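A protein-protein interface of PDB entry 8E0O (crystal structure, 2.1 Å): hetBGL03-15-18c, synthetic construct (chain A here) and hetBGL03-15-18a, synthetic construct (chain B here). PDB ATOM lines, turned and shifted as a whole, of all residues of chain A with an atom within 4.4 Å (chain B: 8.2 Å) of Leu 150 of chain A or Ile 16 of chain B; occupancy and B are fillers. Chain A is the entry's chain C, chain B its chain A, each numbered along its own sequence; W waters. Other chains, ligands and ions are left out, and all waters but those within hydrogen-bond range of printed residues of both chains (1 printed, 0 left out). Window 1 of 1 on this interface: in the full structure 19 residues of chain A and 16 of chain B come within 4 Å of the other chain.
A ring nitrogen (ND1) of His 15 of chain B is in hydrogen-bond range of the backbone carbonyl oxygen of Glu 11 of chain B (3.2 Å).
Among the printed residues, merely in contact across the chains: Glu 151 of chain A with Ala 32 of chain B (3.4 Å), Leu 154 of chain A with His 35 of chain B (3.5 Å), Leu 154 of chain A with Leu 13 of chain B (3.6 Å), Ile 134 of chain A with Val 19 of chain B (3.6 Å), Leu 146 of chain A with Leu 23 of chain B (3.6 Å), Leu 127 of chain A with His 15 of chain B (3.6 Å), Ile 147 of chain A with Leu 23 of chain B (3.6 Å), Leu 154 of chain A with Ile 16 of chain B (3.6 Å), Ile 134 of chain A with Leu 23 of chain B (3.6 Å), Leu 154 of chain A with Leu 20 of chain B (3.6 Å), Leu 150 of chain A with Ile 16 of chain B (3.7 Å), Leu 127 of chain A with Ile 16 of chain B (3.7 Å), Ile 147 of chain A with Ala 24 of chain B (3.7 Å), Leu 150 of chain A with Val 19 of chain B (3.7 Å), Leu 127 of chain A with Val 19 of chain B (3.8 Å), Leu 153 of chain A with Ile 16 of chain B (3.9 Å) and Leu 150 of chain A with Leu 20 of chain B (3.95 Å).
Of chain B, only Ile 16, Val 19 and Leu 20 come within 4 Å of Leu 150 of chain A. No residue of chain B comes within 4 Å of Arg 149 of chain A. Of the printed residues of chain A, Val 19 of chain B touches Leu 127, Ile 134 and Leu 150. Printed residues of chain B within 4 Å of Leu 127 of chain A: His 15 (3.6 Å), Ile 16 (3.7 Å) and Val 19 (3.8 Å). Printed residues of chain A within 4 Å of Leu 23 of chain B: Ile 134 (3.6 Å), Leu 146 (3.6 Å) and Ile 147 (3.6 Å). Of the printed residues of chain B, Ile 147 of chain A touches Leu 23 and Ala 24. Val 76 of chain B touches none of the printed residues of chain A. Val 14 of chain B touches none of the printed residues of chain A. The nearest printed residue of chain A that does not touch Ile 16 of chain B is Glu 151 of chain A (5.7 Å). The nearest printed residue of chain B that does not touch Ile 147 of chain A is Leu 20 of chain B (4.1 Å).
Printed residues of chain B that touch a printed residue of chain A: Leu 13, His 15, Ile 16, Val 19, Leu 20, Leu 23, Ala 24, Ala 32 and His 35. Hydrophobic or aromatic side chains of chain B within 4 Å of the printed part of chain A: Leu 13, His 15, Ile 16, Val 19, Leu 20, Leu 23, Ala 32 and His 35. Of the 12 printed residues of chain A, 8 touch a printed residue of chain B. Printed residues of chain A that touch a printed residue of chain B: Leu 127, Ile 134, Leu 146, Ile 147, Leu 150, Glu 151, Leu 153 and Leu 154. Along chain A the printed residues that touch a printed residue of chain B span positions 127 to 154. Among the printed residues, no Asp or Glu carboxylate lies within 4 Å of a Lys or Arg side-chain nitrogen of the other chain.
Water W1 bridges OE2 of Glu 151 of chain A (2.4 Å) and ND1 of His 35 of chain B (2.6 Å).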
ATOM      1  N   LEU A 127       0.679 -19.934  27.150  1.00  0.00           N
ATOM      2  CA  LEU A 127       0.239 -20.763  26.033  1.00  0.00           C
ATOM      3  C   LEU A 127      -0.947 -20.137  25.312  1.00  0.00           C
ATOM      4  O   LEU A 127      -1.001 -20.141  24.076  1.00  0.00           O
ATOM      5  CB  LEU A 127      -0.116 -22.164  26.531  1.00  0.00           C
ATOM      6  CG  LEU A 127      -0.680 -23.128  25.485  1.00  0.00           C
ATOM      7  CD1 LEU A 127       0.310 -23.323  24.348  1.00  0.00           C
ATOM      8  CD2 LEU A 127      -1.046 -24.460  26.124  1.00  0.00           C
ATOM      9  N   ILE A 130       0.143 -17.436  23.025  1.00  0.00           N
ATOM     10  CA  ILE A 130       0.820 -17.944  21.837  1.00  0.00           C
ATOM     11  C   ILE A 130      -0.199 -18.443  20.818  1.00  0.00           C
ATOM     12  O   ILE A 130      -0.009 -18.295  19.604  1.00  0.00           O
ATOM     13  CB  ILE A 130       1.828 -19.039  22.233  1.00  0.00           C
ATOM     14  CG1 ILE A 130       3.062 -18.413  22.886  1.00  0.00           C
ATOM     15  CG2 ILE A 130       2.247 -19.861  21.029  1.00  0.00           C
ATOM     16  CD1 ILE A 130       3.953 -19.415  23.590  1.00  0.00           C
ATOM     17  N   ILE A 134      -0.564 -17.746  16.938  1.00  0.00           N
ATOM     18  CA  ILE A 134      -0.522 -18.869  16.007  1.00  0.00           C
ATOM     19  C   ILE A 134      -1.791 -18.932  15.165  1.00  0.00           C
ATOM     20  O   ILE A 134      -1.740 -19.319  13.989  1.00  0.00           O
ATOM     21  CB  ILE A 134      -0.281 -20.182  16.773  1.00  0.00           C
ATOM     22  CG1 ILE A 134       1.199 -20.313  17.137  1.00  0.00           C
ATOM     23  CG2 ILE A 134      -0.737 -21.390  15.966  1.00  0.00           C
ATOM     24  CD1 ILE A 134       1.508 -21.537  17.949  1.00  0.00           C
ATOM     25  N   LEU A 146       7.805 -19.309  17.039  1.00  0.00           N
ATOM     26  CA  LEU A 146       6.773 -19.791  17.949  1.00  0.00           C
ATOM     27  C   LEU A 146       6.991 -21.253  18.317  1.00  0.00           C
ATOM     28  O   LEU A 146       6.624 -21.673  19.420  1.00  0.00           O
ATOM     29  CB  LEU A 146       5.393 -19.589  17.322  1.00  0.00           C
ATOM     30  CG  LEU A 146       4.904 -18.139  17.276  1.00  0.00           C
ATOM     31  CD1 LEU A 146       3.776 -17.981  16.271  1.00  0.00           C
ATOM     32  CD2 LEU A 146       4.459 -17.681  18.656  1.00  0.00           C
ATOM     33  N   ILE A 147       7.586 -22.038  17.416  1.00  0.00           N
ATOM     34  CA  ILE A 147       7.927 -23.419  17.744  1.00  0.00           C
ATOM     35  C   ILE A 147       8.990 -23.457  18.837  1.00  0.00           C
ATOM     36  O   ILE A 147       8.904 -24.255  19.778  1.00  0.00           O
ATOM     37  CB  ILE A 147       8.381 -24.173  16.479  1.00  0.00           C
ATOM     38  CG1 ILE A 147       7.172 -24.732  15.726  1.00  0.00           C
ATOM     39  CG2 ILE A 147       9.351 -25.295  16.830  1.00  0.00           C
ATOM     40  CD1 ILE A 147       7.515 -25.332  14.381  1.00  0.00           C
ATOM     41  N   ARG A 148      10.001 -22.591  18.735  1.00  0.00           N
ATOM     42  CA  ARG A 148      11.038 -22.541  19.760  1.00  0.00           C
ATOM     43  C   ARG A 148      10.468 -22.092  21.099  1.00  0.00           C
ATOM     44  O   ARG A 148      10.858 -22.608  22.153  1.00  0.00           O
ATOM     45  CB  ARG A 148      12.168 -21.611  19.317  1.00  0.00           C
ATOM     46  N   ARG A 149       9.543 -21.130  21.079  1.00  0.00           N
ATOM     47  CA  ARG A 149       8.917 -20.682  22.319  1.00  0.00           C
ATOM     48  C   ARG A 149       8.062 -21.783  22.933  1.00  0.00           C
ATOM     49  O   ARG A 149       8.006 -21.922  24.160  1.00  0.00           O
ATOM     50  CB  ARG A 149       8.081 -19.428  22.063  1.00  0.00           C
ATOM     51  N   LEU A 150       7.386 -22.574  22.095  1.00  0.00           N
ATOM     52  CA  LEU A 150       6.602 -23.691  22.610  1.00  0.00           C
ATOM     53  C   LEU A 150       7.504 -24.794  23.148  1.00  0.00           C
ATOM     54  O   LEU A 150       7.184 -25.426  24.161  1.00  0.00           O
ATOM     55  CB  LEU A 150       5.681 -24.235  21.518  1.00  0.00           C
ATOM     56  CG  LEU A 150       4.439 -23.396  21.212  1.00  0.00           C
ATOM     57  CD1 LEU A 150       3.915 -23.702  19.817  1.00  0.00           C
ATOM     58  CD2 LEU A 150       3.364 -23.631  22.261  1.00  0.00           C
ATOM     59  N   GLU A 151       8.634 -25.044  22.481  1.00  0.00           N
ATOM     60  CA  GLU A 151       9.572 -26.049  22.968  1.00  0.00           C
ATOM     61  C   GLU A 151      10.183 -25.631  24.298  1.00  0.00           C
ATOM     62  O   GLU A 151      10.344 -26.460  25.202  1.00  0.00           O
ATOM     63  CB  GLU A 151      10.665 -26.297  21.929  1.00  0.00           C
ATOM     64  CG  GLU A 151      10.340 -27.401  20.940  1.00  0.00           C
ATOM     65  CD  GLU A 151      11.179 -27.322  19.679  1.00  0.00           C
ATOM     66  OE1 GLU A 151      11.820 -26.276  19.453  1.00  0.00           O
ATOM     67  OE2 GLU A 151      11.198 -28.310  18.915  1.00  0.00           O
ATOM     68  N   GLU A 152      10.533 -24.350  24.436  1.00  0.00           N
ATOM     69  CA  GLU A 152      11.022 -23.856  25.718  1.00  0.00           C
ATOM     70  C   GLU A 152       9.929 -23.915  26.777  1.00  0.00           C
ATOM     71  O   GLU A 152      10.202 -24.200  27.949  1.00  0.00           O
ATOM     72  CB  GLU A 152      11.551 -22.429  25.565  1.00  0.00           C
ATOM     73  N   LEU A 153       8.682 -23.650  26.380  1.00  0.00           N
ATOM     74  CA  LEU A 153       7.563 -23.805  27.304  1.00  0.00           C
ATOM     75  C   LEU A 153       7.415 -25.255  27.745  1.00  0.00           C
ATOM     76  O   LEU A 153       7.062 -25.528  28.899  1.00  0.00           O
ATOM     77  CB  LEU A 153       6.273 -23.308  26.650  1.00  0.00           C
ATOM     78  CG  LEU A 153       5.368 -22.401  27.485  1.00  0.00           C
ATOM     79  CD1 LEU A 153       6.176 -21.302  28.156  1.00  0.00           C
ATOM     80  CD2 LEU A 153       4.261 -21.811  26.622  1.00  0.00           C
ATOM     81  N   LEU A 154       7.686 -26.199  26.840  1.00  0.00           N
ATOM     82  CA  LEU A 154       7.632 -27.614  27.193  1.00  0.00           C
ATOM     83  C   LEU A 154       8.656 -27.947  28.271  1.00  0.00           C
ATOM     84  O   LEU A 154       8.344 -28.634  29.252  1.00  0.00           O
ATOM     85  CB  LEU A 154       7.872 -28.475  25.951  1.00  0.00           C
ATOM     86  CG  LEU A 154       6.666 -29.075  25.229  1.00  0.00           C
ATOM     87  CD1 LEU A 154       7.122 -30.033  24.141  1.00  0.00           C
ATOM     88  CD2 LEU A 154       5.734 -29.773  26.202  1.00  0.00           C
ATOM     89  N   ASN B   9      -0.017 -30.044  35.972  1.00  0.00           N
ATOM     90  CA  ASN B   9       1.122 -29.910  35.070  1.00  0.00           C
ATOM     91  C   ASN B   9       0.965 -30.804  33.846  1.00  0.00           C
ATOM     92  O   ASN B   9       1.362 -30.423  32.738  1.00  0.00           O
ATOM     93  CB  ASN B   9       2.418 -30.236  35.810  1.00  0.00           C
ATOM     94  CG  ASN B   9       3.642 -30.105  34.925  1.00  0.00           C
ATOM     95  OD1 ASN B   9       4.058 -28.999  34.580  1.00  0.00           O
ATOM     96  ND2 ASN B   9       4.227 -31.238  34.554  1.00  0.00           N
ATOM     97  N   LEU B  10       0.387 -31.996  34.023  1.00  0.00           N
ATOM     98  CA  LEU B  10       0.198 -32.898  32.893  1.00  0.00           C
ATOM     99  C   LEU B  10      -0.800 -32.331  31.892  1.00  0.00           C
ATOM    100  O   LEU B  10      -0.612 -32.466  30.677  1.00  0.00           O
ATOM    101  CB  LEU B  10      -0.258 -34.272  33.386  1.00  0.00           C
ATOM    102  CG  LEU B  10       0.788 -35.107  34.128  1.00  0.00           C
ATOM    103  CD1 LEU B  10       0.200 -36.433  34.586  1.00  0.00           C
ATOM    104  CD2 LEU B  10       2.016 -35.332  33.257  1.00  0.00           C
ATOM    105  N   GLU B  11      -1.867 -31.693  32.379  1.00  0.00           N
ATOM    106  CA  GLU B  11      -2.840 -31.090  31.473  1.00  0.00           C
ATOM    107  C   GLU B  11      -2.222 -29.939  30.689  1.00  0.00           C
ATOM    108  O   GLU B  11      -2.478 -29.790  29.489  1.00  0.00           O
ATOM    109  CB  GLU B  11      -4.062 -30.609  32.253  1.00  0.00           C
ATOM    110  CG  GLU B  11      -5.133 -29.979  31.379  1.00  0.00           C
ATOM    111  CD  GLU B  11      -6.401 -29.669  32.144  1.00  0.00           C
ATOM    112  OE1 GLU B  11      -6.313 -29.403  33.361  1.00  0.00           O
ATOM    113  OE2 GLU B  11      -7.486 -29.693  31.526  1.00  0.00           O
ATOM    114  N   LEU B  12      -1.412 -29.110  31.353  1.00  0.00           N
ATOM    115  CA  LEU B  12      -0.694 -28.060  30.641  1.00  0.00           C
ATOM    116  C   LEU B  12       0.298 -28.654  29.650  1.00  0.00           C
ATOM    117  O   LEU B  12       0.473 -28.130  28.543  1.00  0.00           O
ATOM    118  CB  LEU B  12       0.020 -27.147  31.639  1.00  0.00           C
ATOM    119  CG  LEU B  12       1.041 -26.162  31.066  1.00  0.00           C
ATOM    120  CD1 LEU B  12       0.349 -25.076  30.255  1.00  0.00           C
ATOM    121  CD2 LEU B  12       1.879 -25.557  32.181  1.00  0.00           C
ATOM    122  N   LEU B  13       0.946 -29.758  30.027  1.00  0.00           N
ATOM    123  CA  LEU B  13       1.932 -30.390  29.154  1.00  0.00           C
ATOM    124  C   LEU B  13       1.297 -30.853  27.848  1.00  0.00           C
ATOM    125  O   LEU B  13       1.842 -30.620  26.762  1.00  0.00           O
ATOM    126  CB  LEU B  13       2.586 -31.567  29.878  1.00  0.00           C
ATOM    127  CG  LEU B  13       3.959 -31.352  30.515  1.00  0.00           C
ATOM    128  CD1 LEU B  13       4.564 -32.683  30.934  1.00  0.00           C
ATOM    129  CD2 LEU B  13       4.887 -30.620  29.566  1.00  0.00           C
ATOM    130  N   VAL B  14       0.139 -31.512  27.935  1.00  0.00           N
ATOM    131  CA  VAL B  14      -0.488 -32.045  26.730  1.00  0.00           C
ATOM    132  C   VAL B  14      -1.098 -30.926  25.892  1.00  0.00           C
ATOM    133  O   VAL B  14      -1.226 -31.058  24.669  1.00  0.00           O
ATOM    134  CB  VAL B  14      -1.528 -33.122  27.099  1.00  0.00           C
ATOM    135  CG1 VAL B  14      -2.784 -32.493  27.684  1.00  0.00           C
ATOM    136  CG2 VAL B  14      -1.865 -33.977  25.884  1.00  0.00           C
ATOM    137  N   HIS B  15      -1.470 -29.807  26.518  1.00  0.00           N
ATOM    138  CA  HIS B  15      -1.995 -28.682  25.754  1.00  0.00           C
ATOM    139  C   HIS B  15      -0.889 -27.910  25.048  1.00  0.00           C
ATOM    140  O   HIS B  15      -1.122 -27.347  23.972  1.00  0.00           O
ATOM    141  CB  HIS B  15      -2.804 -27.757  26.663  1.00  0.00           C
ATOM    142  CG  HIS B  15      -4.169 -28.279  26.986  1.00  0.00           C
ATOM    143  ND1 HIS B  15      -4.824 -27.977  28.161  1.00  0.00           N
ATOM    144  CD2 HIS B  15      -5.001 -29.089  26.289  1.00  0.00           C
ATOM    145  CE1 HIS B  15      -6.002 -28.576  28.172  1.00  0.00           C
ATOM    146  NE2 HIS B  15      -6.133 -29.256  27.047  1.00  0.00           N
ATOM    147  N   ILE B  16       0.312 -27.867  25.632  1.00  0.00           N
ATOM    148  CA  ILE B  16       1.463 -27.343  24.903  1.00  0.00           C
ATOM    149  C   ILE B  16       1.807 -28.260  23.738  1.00  0.00           C
ATOM    150  O   ILE B  16       2.109 -27.797  22.631  1.00  0.00           O
ATOM    151  CB  ILE B  16       2.662 -27.160  25.849  1.00  0.00           C
ATOM    152  CG1 ILE B  16       2.346 -26.129  26.933  1.00  0.00           C
ATOM    153  CG2 ILE B  16       3.896 -26.733  25.071  1.00  0.00           C
ATOM    154  CD1 ILE B  16       3.314 -26.162  28.096  1.00  0.00           C
ATOM    155  N   ALA B  17       1.757 -29.575  23.966  1.00  0.00           N
ATOM    156  CA  ALA B  17       2.063 -30.529  22.906  1.00  0.00           C
ATOM    157  C   ALA B  17       1.052 -30.439  21.770  1.00  0.00           C
ATOM    158  O   ALA B  17       1.409 -30.598  20.597  1.00  0.00           O
ATOM    159  CB  ALA B  17       2.108 -31.946  23.475  1.00  0.00           C
ATOM    160  N   GLU B  18      -0.218 -30.187  22.100  1.00  0.00           N
ATOM    161  CA  GLU B  18      -1.237 -30.043  21.064  1.00  0.00           C
ATOM    162  C   GLU B  18      -0.937 -28.852  20.166  1.00  0.00           C
ATOM    163  O   GLU B  18      -0.994 -28.954  18.934  1.00  0.00           O
ATOM    164  CB  GLU B  18      -2.618 -29.901  21.704  1.00  0.00           C
ATOM    165  CG  GLU B  18      -3.741 -29.682  20.703  1.00  0.00           C
ATOM    166  CD  GLU B  18      -5.082 -29.447  21.369  1.00  0.00           C
ATOM    167  OE1 GLU B  18      -5.102 -29.148  22.582  1.00  0.00           O
ATOM    168  OE2 GLU B  18      -6.118 -29.562  20.682  1.00  0.00           O
ATOM    169  N   VAL B  19      -0.609 -27.708  20.769  1.00  0.00           N
ATOM    170  CA  VAL B  19      -0.294 -26.516  19.987  1.00  0.00           C
ATOM    171  C   VAL B  19       1.010 -26.707  19.223  1.00  0.00           C
ATOM    172  O   VAL B  19       1.126 -26.306  18.059  1.00  0.00           O
ATOM    173  CB  VAL B  19      -0.242 -25.283  20.908  1.00  0.00           C
ATOM    174  CG1 VAL B  19       0.197 -24.055  20.132  1.00  0.00           C
ATOM    175  CG2 VAL B  19      -1.598 -25.051  21.556  1.00  0.00           C
ATOM    176  N   LEU B  20       2.005 -27.334  19.856  1.00  0.00           N
ATOM    177  CA  LEU B  20       3.284 -27.555  19.188  1.00  0.00           C
ATOM    178  C   LEU B  20       3.136 -28.503  18.006  1.00  0.00           C
ATOM    179  O   LEU B  20       3.702 -28.262  16.933  1.00  0.00           O
ATOM    180  CB  LEU B  20       4.311 -28.095  20.184  1.00  0.00           C
ATOM    181  CG  LEU B  20       5.668 -28.489  19.595  1.00  0.00           C
ATOM    182  CD1 LEU B  20       6.347 -27.291  18.943  1.00  0.00           C
ATOM    183  CD2 LEU B  20       6.559 -29.101  20.661  1.00  0.00           C
ATOM    184  N   ALA B  21       2.382 -29.591  18.181  1.00  0.00           N
ATOM    185  CA  ALA B  21       2.177 -30.529  17.083  1.00  0.00           C
ATOM    186  C   ALA B  21       1.437 -29.871  15.927  1.00  0.00           C
ATOM    187  O   ALA B  21       1.745 -30.124  14.757  1.00  0.00           O
ATOM    188  CB  ALA B  21       1.414 -31.759  17.574  1.00  0.00           C
ATOM    189  N   ARG B  22       0.456 -29.020  16.238  1.00  0.00           N
ATOM    190  CA  ARG B  22      -0.285 -28.324  15.191  1.00  0.00           C
ATOM    191  C   ARG B  22       0.630 -27.417  14.380  1.00  0.00           C
ATOM    192  O   ARG B  22       0.549 -27.383  13.146  1.00  0.00           O
ATOM    193  CB  ARG B  22      -1.426 -27.520  15.813  1.00  0.00           C
ATOM    194  CG  ARG B  22      -2.366 -26.873  14.809  1.00  0.00           C
ATOM    195  CD  ARG B  22      -3.681 -26.489  15.472  1.00  0.00           C
ATOM    196  NE  ARG B  22      -3.477 -25.993  16.828  1.00  0.00           N
ATOM    197  CZ  ARG B  22      -4.345 -26.138  17.820  1.00  0.00           C
ATOM    198  NH1 ARG B  22      -5.498 -26.764  17.645  1.00  0.00           N
ATOM    199  NH2 ARG B  22      -4.048 -25.645  19.020  1.00  0.00           N
ATOM    200  N   LEU B  23       1.515 -26.682  15.055  1.00  0.00           N
ATOM    201  CA  LEU B  23       2.398 -25.756  14.357  1.00  0.00           C
ATOM    202  C   LEU B  23       3.559 -26.480  13.687  1.00  0.00           C
ATOM    203  O   LEU B  23       3.951 -26.124  12.571  1.00  0.00           O
ATOM    204  CB  LEU B  23       2.916 -24.697  15.331  1.00  0.00           C
ATOM    205  CG  LEU B  23       3.594 -23.479  14.703  1.00  0.00           C
ATOM    206  CD1 LEU B  23       2.600 -22.672  13.881  1.00  0.00           C
ATOM    207  CD2 LEU B  23       4.230 -22.615  15.776  1.00  0.00           C
ATOM    208  N   ALA B  24       4.122 -27.495  14.348  1.00  0.00           N
ATOM    209  CA  ALA B  24       5.248 -28.221  13.768  1.00  0.00           C
ATOM    210  C   ALA B  24       4.844 -28.929  12.481  1.00  0.00           C
ATOM    211  O   ALA B  24       5.620 -28.976  11.519  1.00  0.00           O
ATOM    212  CB  ALA B  24       5.808 -29.223  14.777  1.00  0.00           C
ATOM    213  N   ALA B  32      10.109 -31.627  16.009  1.00  0.00           N
ATOM    214  CA  ALA B  32       9.198 -30.997  16.958  1.00  0.00           C
ATOM    215  C   ALA B  32       7.846 -31.698  16.980  1.00  0.00           C
ATOM    216  O   ALA B  32       7.204 -31.772  18.033  1.00  0.00           O
ATOM    217  CB  ALA B  32       9.027 -29.516  16.623  1.00  0.00           C
ATOM    218  N   HIS B  35       8.358 -34.904  18.893  1.00  0.00           N
ATOM    219  CA  HIS B  35       8.503 -34.554  20.302  1.00  0.00           C
ATOM    220  C   HIS B  35       7.146 -34.277  20.940  1.00  0.00           C
ATOM    221  O   HIS B  35       6.872 -34.734  22.056  1.00  0.00           O
ATOM    222  CB  HIS B  35       9.422 -33.341  20.444  1.00  0.00           C
ATOM    223  CG  HIS B  35       9.665 -32.924  21.862  1.00  0.00           C
ATOM    224  ND1 HIS B  35      10.077 -31.652  22.202  1.00  0.00           N
ATOM    225  CD2 HIS B  35       9.562 -33.610  23.025  1.00  0.00           C
ATOM    226  CE1 HIS B  35      10.212 -31.572  23.513  1.00  0.00           C
ATOM    227  NE2 HIS B  35       9.906 -32.745  24.036  1.00  0.00           N
ATOM    228  N   ALA B  36       6.284 -33.534  20.243  1.00  0.00           N
ATOM    229  CA  ALA B  36       4.952 -33.259  20.772  1.00  0.00           C
ATOM    230  C   ALA B  36       4.133 -34.538  20.893  1.00  0.00           C
ATOM    231  O   ALA B  36       3.335 -34.688  21.825  1.00  0.00           O
ATOM    232  CB  ALA B  36       4.235 -32.242  19.886  1.00  0.00           C
ATOM    233  N   VAL B  39       5.290 -36.437  24.089  1.00  0.00           N
ATOM    234  CA  VAL B  39       4.820 -35.822  25.325  1.00  0.00           C
ATOM    235  C   VAL B  39       3.348 -36.142  25.557  1.00  0.00           C
ATOM    236  O   VAL B  39       2.938 -36.472  26.676  1.00  0.00           O
ATOM    237  CB  VAL B  39       5.079 -34.305  25.298  1.00  0.00           C
ATOM    238  CG1 VAL B  39       4.414 -33.625  26.486  1.00  0.00           C
ATOM    239  CG2 VAL B  39       6.574 -34.025  25.286  1.00  0.00           C
ATOM    240  N   ALA B  40       2.531 -36.058  24.503  1.00  0.00           N
ATOM    241  CA  ALA B  40       1.115 -36.384  24.642  1.00  0.00           C
ATOM    242  C   ALA B  40       0.922 -37.847  25.023  1.00  0.00           C
ATOM    243  O   ALA B  40       0.008 -38.182  25.787  1.00  0.00           O
ATOM    244  CB  ALA B  40       0.372 -36.062  23.346  1.00  0.00           C
ATOM    245  N   VAL B  76      -5.934 -35.421  22.004  1.00  0.00           N
ATOM    246  CA  VAL B  76      -4.805 -34.749  21.364  1.00  0.00           C
ATOM    247  C   VAL B  76      -3.981 -35.742  20.554  1.00  0.00           C
ATOM    248  O   VAL B  76      -3.574 -35.457  19.421  1.00  0.00           O
ATOM    249  CB  VAL B  76      -3.945 -34.031  22.422  1.00  0.00           C
ATOM    250  CG1 VAL B  76      -2.649 -33.528  21.807  1.00  0.00           C
ATOM    251  CG2 VAL B  76      -4.725 -32.884  23.051  1.00  0.00           C
HETATM  252  O   HOH W   1      10.882 -30.460  20.005  1.00  0.00           O
